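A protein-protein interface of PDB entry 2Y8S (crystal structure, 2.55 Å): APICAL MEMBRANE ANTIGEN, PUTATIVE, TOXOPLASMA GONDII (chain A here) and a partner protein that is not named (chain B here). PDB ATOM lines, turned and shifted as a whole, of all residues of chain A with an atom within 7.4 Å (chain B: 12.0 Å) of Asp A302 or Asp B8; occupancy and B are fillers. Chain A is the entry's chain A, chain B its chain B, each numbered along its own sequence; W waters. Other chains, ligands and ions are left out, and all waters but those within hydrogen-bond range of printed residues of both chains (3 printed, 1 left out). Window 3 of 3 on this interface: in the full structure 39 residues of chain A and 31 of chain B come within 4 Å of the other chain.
Of the printed residues of chain B, Leu A41 touches Ile B9 and Gly B10. Of chain B, only Glu B7 (3.3 Å) and Asp B8 (2.8 Å) come within 4 Å of Arg A53. Printed residues of chain B within 4 Å of Met A175: Ile B9, Gly B10 and Gly B11. Gln A280 touches just one residue of chain B: Ile B9 (3.5 Å). Of the printed residues of chain B, Pro A281 touches Asp B8. Of chain B, only Asp B8 comes within 4 Å of Gln A303. Of the printed residues of chain A, Glu B7 touches Leu A51 and Arg A53. Printed residues of chain A within 4 Å of Gly B10: Leu A41 and Met A175. Ala B12 touches none of the printed residues of chain A. The nearest residue of chain B that does not touch Asp A302 is Gln B4 (5.8 Å). The nearest printed residue of chain B that does not touch Met A175 is Met B6 (4.5 Å).
Of the 13 printed residues of chain B, 5 touch a printed residue of chain A. Hydrophobic or aromatic side chains of chain B that line the printed part of chain A: Ile B9. Along chain B the printed residues that touch a printed residue of chain A span positions 7 to 11. Of the 12 printed residues of chain A, 8 touch a printed residue of chain B. Printed residues of chain A that touch a printed residue of chain B: Leu A41, Leu A51, Arg A53, Met A175, Gln A280, Pro A281, Asp A302 and Gln A303. Hydrophobic or aromatic side chains of chain A within 4 Å of the printed part of chain B: Leu A41, Met A175 and Pro A281. Among the printed residues, 12 pairs touch across the chains. Among the printed residues, no Asp or Glu carboxylate lies within 4 Å of a Lys or Arg side-chain nitrogen of the other chain.
Among the printed residues, merely in contact across the chains: Met A175 with Ile B9 (3.1 Å), Pro A281 with Asp B8 (3.3 Å), Arg A53 with Glu B7 (3.3 Å), Gln A280 with Ile B9 (3.5 Å), Met A175 with Gly B11 (3.5 Å), Met A175 with Gly B10 (3.5 Å), Asp A302 with Asp B8 (3.6 Å), Leu A41 with Ile B9 (3.7 Å), Leu A41 with Gly B10 (3.7 Å) and Leu A51 with Glu B7 (3.97 Å).
Water W3 lies within hydrogen-bond range of the backbone carbonyl oxygen (O) of Glu B7 (2.6 Å), the backbone carbonyl oxygen (O) of Gly B11 (2.8 Å) and the backbone NH (N) of Arg A53 (3.0 Å). Water W1 bridges O of Ile B9 (2.7 Å) and NE2 of Gln A280 (3.0 Å). Water W2 lies within hydrogen-bond range of O of Gly B10 (2.8 Å), N of Met A175 (3.2 Å) and N of Ala B12 (3.2 Å).
The backbone carbonyl oxygen (O) of Leu A41 lies within hydrogen-bond range of the guanidinium group (NH2) of Arg A53 (3.2 Å). The side-chain carboxylate (OD2) of Asp A279 lies within hydrogen-bond range of the backbone NH (N) of Leu A41. The guanidinium group (NH1) of Arg A53 lies within hydrogen-bond range of the backbone carbonyl oxygen (O) of Asp A279 (3.0 Å). The guanidinium group (NH2) of Arg A53 lies within hydrogen-bond range of the backbone carbonyl oxygen (O) of Pro A304 (2.9 Å). O of Met B6 sits at hydrogen-bond distance from N of Gly B11, at 2.7 Å.
The guanidinium group (NH1) of Arg A53 lies within hydrogen-bond range of the backbone carbonyl oxygen (O) of Asp B8. NE2 of Gln A303 lies within hydrogen-bond range of OD1 of Asp B8 (2.7 Å).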
ATOM      1  N   VAL A  39      -8.420  -1.978  15.146  1.00  0.00           N
ATOM      2  CA  VAL A  39      -9.007  -2.972  16.030  1.00  0.00           C
ATOM      3  C   VAL A  39      -7.979  -3.206  17.137  1.00  0.00           C
ATOM      4  O   VAL A  39      -6.878  -3.689  16.887  1.00  0.00           O
ATOM      5  CB  VAL A  39      -9.308  -4.325  15.274  1.00  0.00           C
ATOM      6  CG1 VAL A  39      -9.382  -5.483  16.237  1.00  0.00           C
ATOM      7  CG2 VAL A  39     -10.584  -4.241  14.335  1.00  0.00           C
ATOM      8  N   LEU A  41      -7.093  -5.290  20.174  1.00  0.00           N
ATOM      9  CA  LEU A  41      -7.349  -6.464  20.976  1.00  0.00           C
ATOM     10  C   LEU A  41      -6.044  -6.994  21.536  1.00  0.00           C
ATOM     11  O   LEU A  41      -5.768  -8.174  21.406  1.00  0.00           O
ATOM     12  CB  LEU A  41      -8.101  -7.516  20.164  1.00  0.00           C
ATOM     13  CG  LEU A  41      -9.538  -7.234  19.731  1.00  0.00           C
ATOM     14  CD1 LEU A  41     -10.059  -8.346  18.805  1.00  0.00           C
ATOM     15  CD2 LEU A  41     -10.463  -7.117  20.910  1.00  0.00           C
ATOM     16  N   LEU A  51      -9.887 -17.751  28.226  1.00  0.00           N
ATOM     17  CA  LEU A  51      -9.091 -16.606  27.826  1.00  0.00           C
ATOM     18  C   LEU A  51      -9.939 -15.747  26.911  1.00  0.00           C
ATOM     19  O   LEU A  51     -10.571 -16.282  26.013  1.00  0.00           O
ATOM     20  CB  LEU A  51      -7.848 -17.092  27.091  1.00  0.00           C
ATOM     21  CG  LEU A  51      -6.515 -16.483  27.527  1.00  0.00           C
ATOM     22  CD1 LEU A  51      -6.611 -15.671  28.838  1.00  0.00           C
ATOM     23  CD2 LEU A  51      -5.442 -17.564  27.670  1.00  0.00           C
ATOM     24  N   ARG A  53      -9.905 -11.949  24.651  1.00  0.00           N
ATOM     25  CA  ARG A  53      -9.175 -10.783  24.118  1.00  0.00           C
ATOM     26  C   ARG A  53      -9.693  -9.462  24.686  1.00  0.00           C
ATOM     27  O   ARG A  53     -10.896  -9.200  24.781  1.00  0.00           O
ATOM     28  CB  ARG A  53      -9.209 -10.720  22.583  1.00  0.00           C
ATOM     29  CG  ARG A  53      -8.871 -12.039  21.895  1.00  0.00           C
ATOM     30  CD  ARG A  53      -8.675 -11.842  20.433  1.00  0.00           C
ATOM     31  NE  ARG A  53      -7.397 -11.154  20.217  1.00  0.00           N
ATOM     32  CZ  ARG A  53      -6.923 -10.827  19.023  1.00  0.00           C
ATOM     33  NH1 ARG A  53      -7.641 -11.101  17.925  1.00  0.00           N
ATOM     34  NH2 ARG A  53      -5.738 -10.231  18.931  1.00  0.00           N
ATOM     35  N   MET A 175     -15.511  -6.369  20.697  1.00  0.00           N
ATOM     36  CA  MET A 175     -15.434  -6.559  19.253  1.00  0.00           C
ATOM     37  C   MET A 175     -15.484  -5.220  18.569  1.00  0.00           C
ATOM     38  O   MET A 175     -16.222  -4.329  18.955  1.00  0.00           O
ATOM     39  CB  MET A 175     -16.609  -7.399  18.699  1.00  0.00           C
ATOM     40  CG  MET A 175     -16.654  -8.870  19.135  1.00  0.00           C
ATOM     41  SD  MET A 175     -18.099  -9.783  18.485  1.00  0.00           S
ATOM     42  CE  MET A 175     -19.404  -9.111  19.472  1.00  0.00           C
ATOM     43  N   ASP A 279      -5.473  -5.616  15.269  1.00  0.00           N
ATOM     44  CA  ASP A 279      -5.269  -6.887  15.959  1.00  0.00           C
ATOM     45  C   ASP A 279      -6.261  -7.963  15.531  1.00  0.00           C
ATOM     46  O   ASP A 279      -6.336  -9.033  16.135  1.00  0.00           O
ATOM     47  CB  ASP A 279      -5.269  -6.685  17.465  1.00  0.00           C
ATOM     48  CG  ASP A 279      -4.146  -5.756  17.940  1.00  0.00           C
ATOM     49  OD1 ASP A 279      -3.102  -5.583  17.231  1.00  0.00           O
ATOM     50  OD2 ASP A 279      -4.343  -5.159  19.032  1.00  0.00           O
ATOM     51  N   GLN A 280      -6.995  -7.692  14.465  1.00  0.00           N
ATOM     52  CA  GLN A 280      -8.076  -8.543  14.002  1.00  0.00           C
ATOM     53  C   GLN A 280      -7.470  -9.729  13.258  1.00  0.00           C
ATOM     54  O   GLN A 280      -6.516  -9.538  12.488  1.00  0.00           O
ATOM     55  CB  GLN A 280      -8.903  -7.723  13.026  1.00  0.00           C
ATOM     56  CG  GLN A 280     -10.124  -8.380  12.466  1.00  0.00           C
ATOM     57  CD  GLN A 280     -11.276  -8.468  13.472  1.00  0.00           C
ATOM     58  OE1 GLN A 280     -12.357  -8.920  13.108  1.00  0.00           O
ATOM     59  NE2 GLN A 280     -11.059  -8.010  14.725  1.00  0.00           N
ATOM     60  N   PRO A 281      -8.013 -10.957  13.481  1.00  0.00           N
ATOM     61  CA  PRO A 281      -7.598 -12.210  12.818  1.00  0.00           C
ATOM     62  C   PRO A 281      -7.586 -12.075  11.305  1.00  0.00           C
ATOM     63  O   PRO A 281      -8.380 -11.296  10.783  1.00  0.00           O
ATOM     64  CB  PRO A 281      -8.707 -13.187  13.199  1.00  0.00           C
ATOM     65  CG  PRO A 281      -9.211 -12.675  14.531  1.00  0.00           C
ATOM     66  CD  PRO A 281      -9.109 -11.184  14.444  1.00  0.00           C
ATOM     67  N   ASP A 302      -6.686 -17.582  14.703  1.00  0.00           N
ATOM     68  CA  ASP A 302      -5.634 -16.553  14.615  1.00  0.00           C
ATOM     69  C   ASP A 302      -5.947 -15.259  15.417  1.00  0.00           C
ATOM     70  O   ASP A 302      -7.059 -14.738  15.344  1.00  0.00           O
ATOM     71  CB  ASP A 302      -5.335 -16.240  13.135  1.00  0.00           C
ATOM     72  CG  ASP A 302      -4.246 -15.200  12.958  1.00  0.00           C
ATOM     73  OD1 ASP A 302      -3.200 -15.287  13.648  1.00  0.00           O
ATOM     74  OD2 ASP A 302      -4.445 -14.277  12.140  1.00  0.00           O
ATOM     75  N   GLN A 303      -4.950 -14.776  16.173  1.00  0.00           N
ATOM     76  CA  GLN A 303      -5.064 -13.659  17.132  1.00  0.00           C
ATOM     77  C   GLN A 303      -3.780 -12.827  17.161  1.00  0.00           C
ATOM     78  O   GLN A 303      -2.972 -12.925  18.089  1.00  0.00           O
ATOM     79  CB  GLN A 303      -5.341 -14.170  18.549  1.00  0.00           C
ATOM     80  CG  GLN A 303      -6.531 -15.090  18.630  1.00  0.00           C
ATOM     81  CD  GLN A 303      -6.992 -15.299  20.043  1.00  0.00           C
ATOM     82  OE1 GLN A 303      -6.331 -14.898  20.997  1.00  0.00           O
ATOM     83  NE2 GLN A 303      -8.155 -15.913  20.188  1.00  0.00           N
ATOM     84  N   PRO A 304      -3.589 -12.003  16.130  1.00  0.00           N
ATOM     85  CA  PRO A 304      -2.374 -11.222  16.002  1.00  0.00           C
ATOM     86  C   PRO A 304      -2.327 -10.064  16.970  1.00  0.00           C
ATOM     87  O   PRO A 304      -3.366  -9.554  17.387  1.00  0.00           O
ATOM     88  CB  PRO A 304      -2.451 -10.689  14.573  1.00  0.00           C
ATOM     89  CG  PRO A 304      -3.750 -11.133  14.015  1.00  0.00           C
ATOM     90  CD  PRO A 304      -4.572 -11.712  15.076  1.00  0.00           C
ATOM     91  N   HIS A 305      -1.114  -9.671  17.331  1.00  0.00           N
ATOM     92  CA  HIS A 305      -0.877  -8.484  18.138  1.00  0.00           C
ATOM     93  C   HIS A 305       0.089  -7.610  17.386  1.00  0.00           C
ATOM     94  O   HIS A 305       1.295  -7.894  17.349  1.00  0.00           O
ATOM     95  CB  HIS A 305      -0.332  -8.807  19.561  1.00  0.00           C
ATOM     96  CG  HIS A 305      -1.308  -9.555  20.417  1.00  0.00           C
ATOM     97  ND1 HIS A 305      -0.924 -10.475  21.372  1.00  0.00           N
ATOM     98  CD2 HIS A 305      -2.661  -9.556  20.421  1.00  0.00           C
ATOM     99  CE1 HIS A 305      -1.997 -10.994  21.934  1.00  0.00           C
ATOM    100  NE2 HIS A 305      -3.063 -10.458  21.370  1.00  0.00           N
ATOM    101  N   ASP B   1     -15.832 -23.875  15.158  1.00  0.00           N
ATOM    102  CA  ASP B   1     -16.511 -23.558  16.427  1.00  0.00           C
ATOM    103  C   ASP B   1     -16.805 -22.055  16.485  1.00  0.00           C
ATOM    104  O   ASP B   1     -15.904 -21.216  16.390  1.00  0.00           O
ATOM    105  CB  ASP B   1     -15.615 -23.947  17.581  1.00  0.00           C
ATOM    106  CG  ASP B   1     -16.201 -23.570  18.932  1.00  0.00           C
ATOM    107  OD1 ASP B   1     -17.158 -24.209  19.388  1.00  0.00           O
ATOM    108  OD2 ASP B   1     -15.670 -22.648  19.555  1.00  0.00           O
ATOM    109  N   ILE B   2     -18.075 -21.738  16.680  1.00  0.00           N
ATOM    110  CA  ILE B   2     -18.532 -20.380  16.732  1.00  0.00           C
ATOM    111  C   ILE B   2     -17.952 -19.617  17.932  1.00  0.00           C
ATOM    112  O   ILE B   2     -17.689 -18.416  17.827  1.00  0.00           O
ATOM    113  CB  ILE B   2     -20.102 -20.316  16.668  1.00  0.00           C
ATOM    114  CG1 ILE B   2     -20.597 -18.863  16.667  1.00  0.00           C
ATOM    115  CG2 ILE B   2     -20.767 -21.176  17.743  1.00  0.00           C
ATOM    116  CD1 ILE B   2     -20.135 -18.065  15.417  1.00  0.00           C
ATOM    117  N   VAL B   3     -17.747 -20.317  19.053  1.00  0.00           N
ATOM    118  CA  VAL B   3     -17.163 -19.694  20.243  1.00  0.00           C
ATOM    119  C   VAL B   3     -15.700 -19.290  20.031  1.00  0.00           C
ATOM    120  O   VAL B   3     -15.297 -18.205  20.422  1.00  0.00           O
ATOM    121  CB  VAL B   3     -17.441 -20.485  21.593  1.00  0.00           C
ATOM    122  CG1 VAL B   3     -18.016 -21.820  21.314  1.00  0.00           C
ATOM    123  CG2 VAL B   3     -16.202 -20.596  22.490  1.00  0.00           C
ATOM    124  N   GLN B   4     -14.933 -20.142  19.374  1.00  0.00           N
ATOM    125  CA  GLN B   4     -13.577 -19.794  19.013  1.00  0.00           C
ATOM    126  C   GLN B   4     -13.520 -18.583  18.077  1.00  0.00           C
ATOM    127  O   GLN B   4     -12.719 -17.655  18.283  1.00  0.00           O
ATOM    128  CB  GLN B   4     -12.865 -20.982  18.400  1.00  0.00           C
ATOM    129  CG  GLN B   4     -11.912 -21.585  19.339  1.00  0.00           C
ATOM    130  CD  GLN B   4     -10.696 -20.721  19.415  1.00  0.00           C
ATOM    131  OE1 GLN B   4     -10.013 -20.535  18.402  1.00  0.00           O
ATOM    132  NE2 GLN B   4     -10.430 -20.140  20.592  1.00  0.00           N
ATOM    133  N   HIS B   5     -14.377 -18.590  17.058  1.00  0.00           N
ATOM    134  CA  HIS B   5     -14.467 -17.463  16.168  1.00  0.00           C
ATOM    135  C   HIS B   5     -14.814 -16.169  16.900  1.00  0.00           C
ATOM    136  O   HIS B   5     -14.173 -15.150  16.680  1.00  0.00           O
ATOM    137  CB  HIS B   5     -15.486 -17.705  15.071  1.00  0.00           C
ATOM    138  CG  HIS B   5     -15.518 -16.595  14.079  1.00  0.00           C
ATOM    139  ND1 HIS B   5     -16.588 -15.729  13.962  1.00  0.00           N
ATOM    140  CD2 HIS B   5     -14.569 -16.150  13.218  1.00  0.00           C
ATOM    141  CE1 HIS B   5     -16.315 -14.828  13.033  1.00  0.00           C
ATOM    142  NE2 HIS B   5     -15.097 -15.059  12.571  1.00  0.00           N
ATOM    143  N   MET B   6     -15.825 -16.215  17.760  1.00  0.00           N
ATOM    144  CA  MET B   6     -16.203 -15.046  18.552  1.00  0.00           C
ATOM    145  C   MET B   6     -15.071 -14.526  19.442  1.00  0.00           C
ATOM    146  O   MET B   6     -14.769 -13.345  19.430  1.00  0.00           O
ATOM    147  CB  MET B   6     -17.448 -15.328  19.390  1.00  0.00           C
ATOM    148  CG  MET B   6     -18.695 -15.538  18.558  1.00  0.00           C
ATOM    149  SD  MET B   6     -19.057 -14.070  17.596  1.00  0.00           S
ATOM    150  CE  MET B   6     -19.797 -14.754  16.100  1.00  0.00           C
ATOM    151  N   GLU B   7     -14.441 -15.435  20.184  1.00  0.00           N
ATOM    152  CA  GLU B   7     -13.308 -15.112  21.052  1.00  0.00           C
ATOM    153  C   GLU B   7     -12.229 -14.372  20.272  1.00  0.00           C
ATOM    154  O   GLU B   7     -11.660 -13.376  20.751  1.00  0.00           O
ATOM    155  CB  GLU B   7     -12.743 -16.374  21.691  1.00  0.00           C
ATOM    156  CG  GLU B   7     -13.251 -16.616  23.107  1.00  0.00           C
ATOM    157  CD  GLU B   7     -13.404 -18.124  23.515  1.00  0.00           C
ATOM    158  OE1 GLU B   7     -12.486 -18.990  23.258  1.00  0.00           O
ATOM    159  OE2 GLU B   7     -14.472 -18.419  24.132  1.00  0.00           O
ATOM    160  N   ASP B   8     -12.015 -14.852  19.046  1.00  0.00           N
ATOM    161  CA  ASP B   8     -10.983 -14.376  18.141  1.00  0.00           C
ATOM    162  C   ASP B   8     -11.175 -12.924  17.757  1.00  0.00           C
ATOM    163  O   ASP B   8     -10.221 -12.179  17.627  1.00  0.00           O
ATOM    164  CB  ASP B   8     -10.988 -15.224  16.882  1.00  0.00           C
ATOM    165  CG  ASP B   8     -10.178 -16.499  17.014  1.00  0.00           C
ATOM    166  OD1 ASP B   8      -9.699 -16.836  18.123  1.00  0.00           O
ATOM    167  OD2 ASP B   8     -10.009 -17.164  15.955  1.00  0.00           O
ATOM    168  N   ILE B   9     -12.412 -12.520  17.570  1.00  0.00           N
ATOM    169  CA  ILE B   9     -12.672 -11.168  17.130  1.00  0.00           C
ATOM    170  C   ILE B   9     -13.102 -10.342  18.334  1.00  0.00           C
ATOM    171  O   ILE B   9     -13.756  -9.300  18.166  1.00  0.00           O
ATOM    172  CB  ILE B   9     -13.751 -11.110  15.995  1.00  0.00           C
ATOM    173  CG1 ILE B   9     -15.119 -11.602  16.528  1.00  0.00           C
ATOM    174  CG2 ILE B   9     -13.272 -11.881  14.754  1.00  0.00           C
ATOM    175  CD1 ILE B   9     -16.272 -11.509  15.541  1.00  0.00           C
ATOM    176  N   GLY B  10     -12.754 -10.816  19.534  1.00  0.00           N
ATOM    177  CA  GLY B  10     -12.990 -10.030  20.757  1.00  0.00           C
ATOM    178  C   GLY B  10     -14.326 -10.205  21.481  1.00  0.00           C
ATOM    179  O   GLY B  10     -14.674  -9.406  22.309  1.00  0.00           O
ATOM    180  N   GLY B  11     -15.067 -11.262  21.158  1.00  0.00           N
ATOM    181  CA  GLY B  11     -16.287 -11.635  21.853  1.00  0.00           C
ATOM    182  C   GLY B  11     -16.075 -11.621  23.336  1.00  0.00           C
ATOM    183  O   GLY B  11     -15.037 -12.069  23.828  1.00  0.00           O
ATOM    184  N   ALA B  12     -17.059 -11.094  24.064  1.00  0.00           N
ATOM    185  CA  ALA B  12     -16.828 -10.759  25.467  1.00  0.00           C
ATOM    186  C   ALA B  12     -17.164 -11.886  26.462  1.00  0.00           C
ATOM    187  O   ALA B  12     -17.918 -12.822  26.146  1.00  0.00           O
ATOM    188  CB  ALA B  12     -17.588  -9.515  25.786  1.00  0.00           C
ATOM    189  N   PRO B  13     -16.618 -11.810  27.689  1.00  0.00           N
ATOM    190  CA  PRO B  13     -17.074 -12.843  28.618  1.00  0.00           C
ATOM    191  C   PRO B  13     -18.555 -12.632  28.891  1.00  0.00           C
ATOM    192  O   PRO B  13     -19.019 -11.497  28.897  1.00  0.00           O
ATOM    193  CB  PRO B  13     -16.220 -12.619  29.863  1.00  0.00           C
ATOM    194  CG  PRO B  13     -15.584 -11.277  29.701  1.00  0.00           C
ATOM    195  CD  PRO B  13     -15.719 -10.810  28.312  1.00  0.00           C
HETATM  196  O   HOH W   1     -13.252  -7.191  16.569  1.00  0.00           O
HETATM  197  O   HOH W   2     -17.119  -8.165  22.738  1.00  0.00           O
HETATM  198  O   HOH W   3     -12.343 -12.578  23.097  1.00  0.00           O
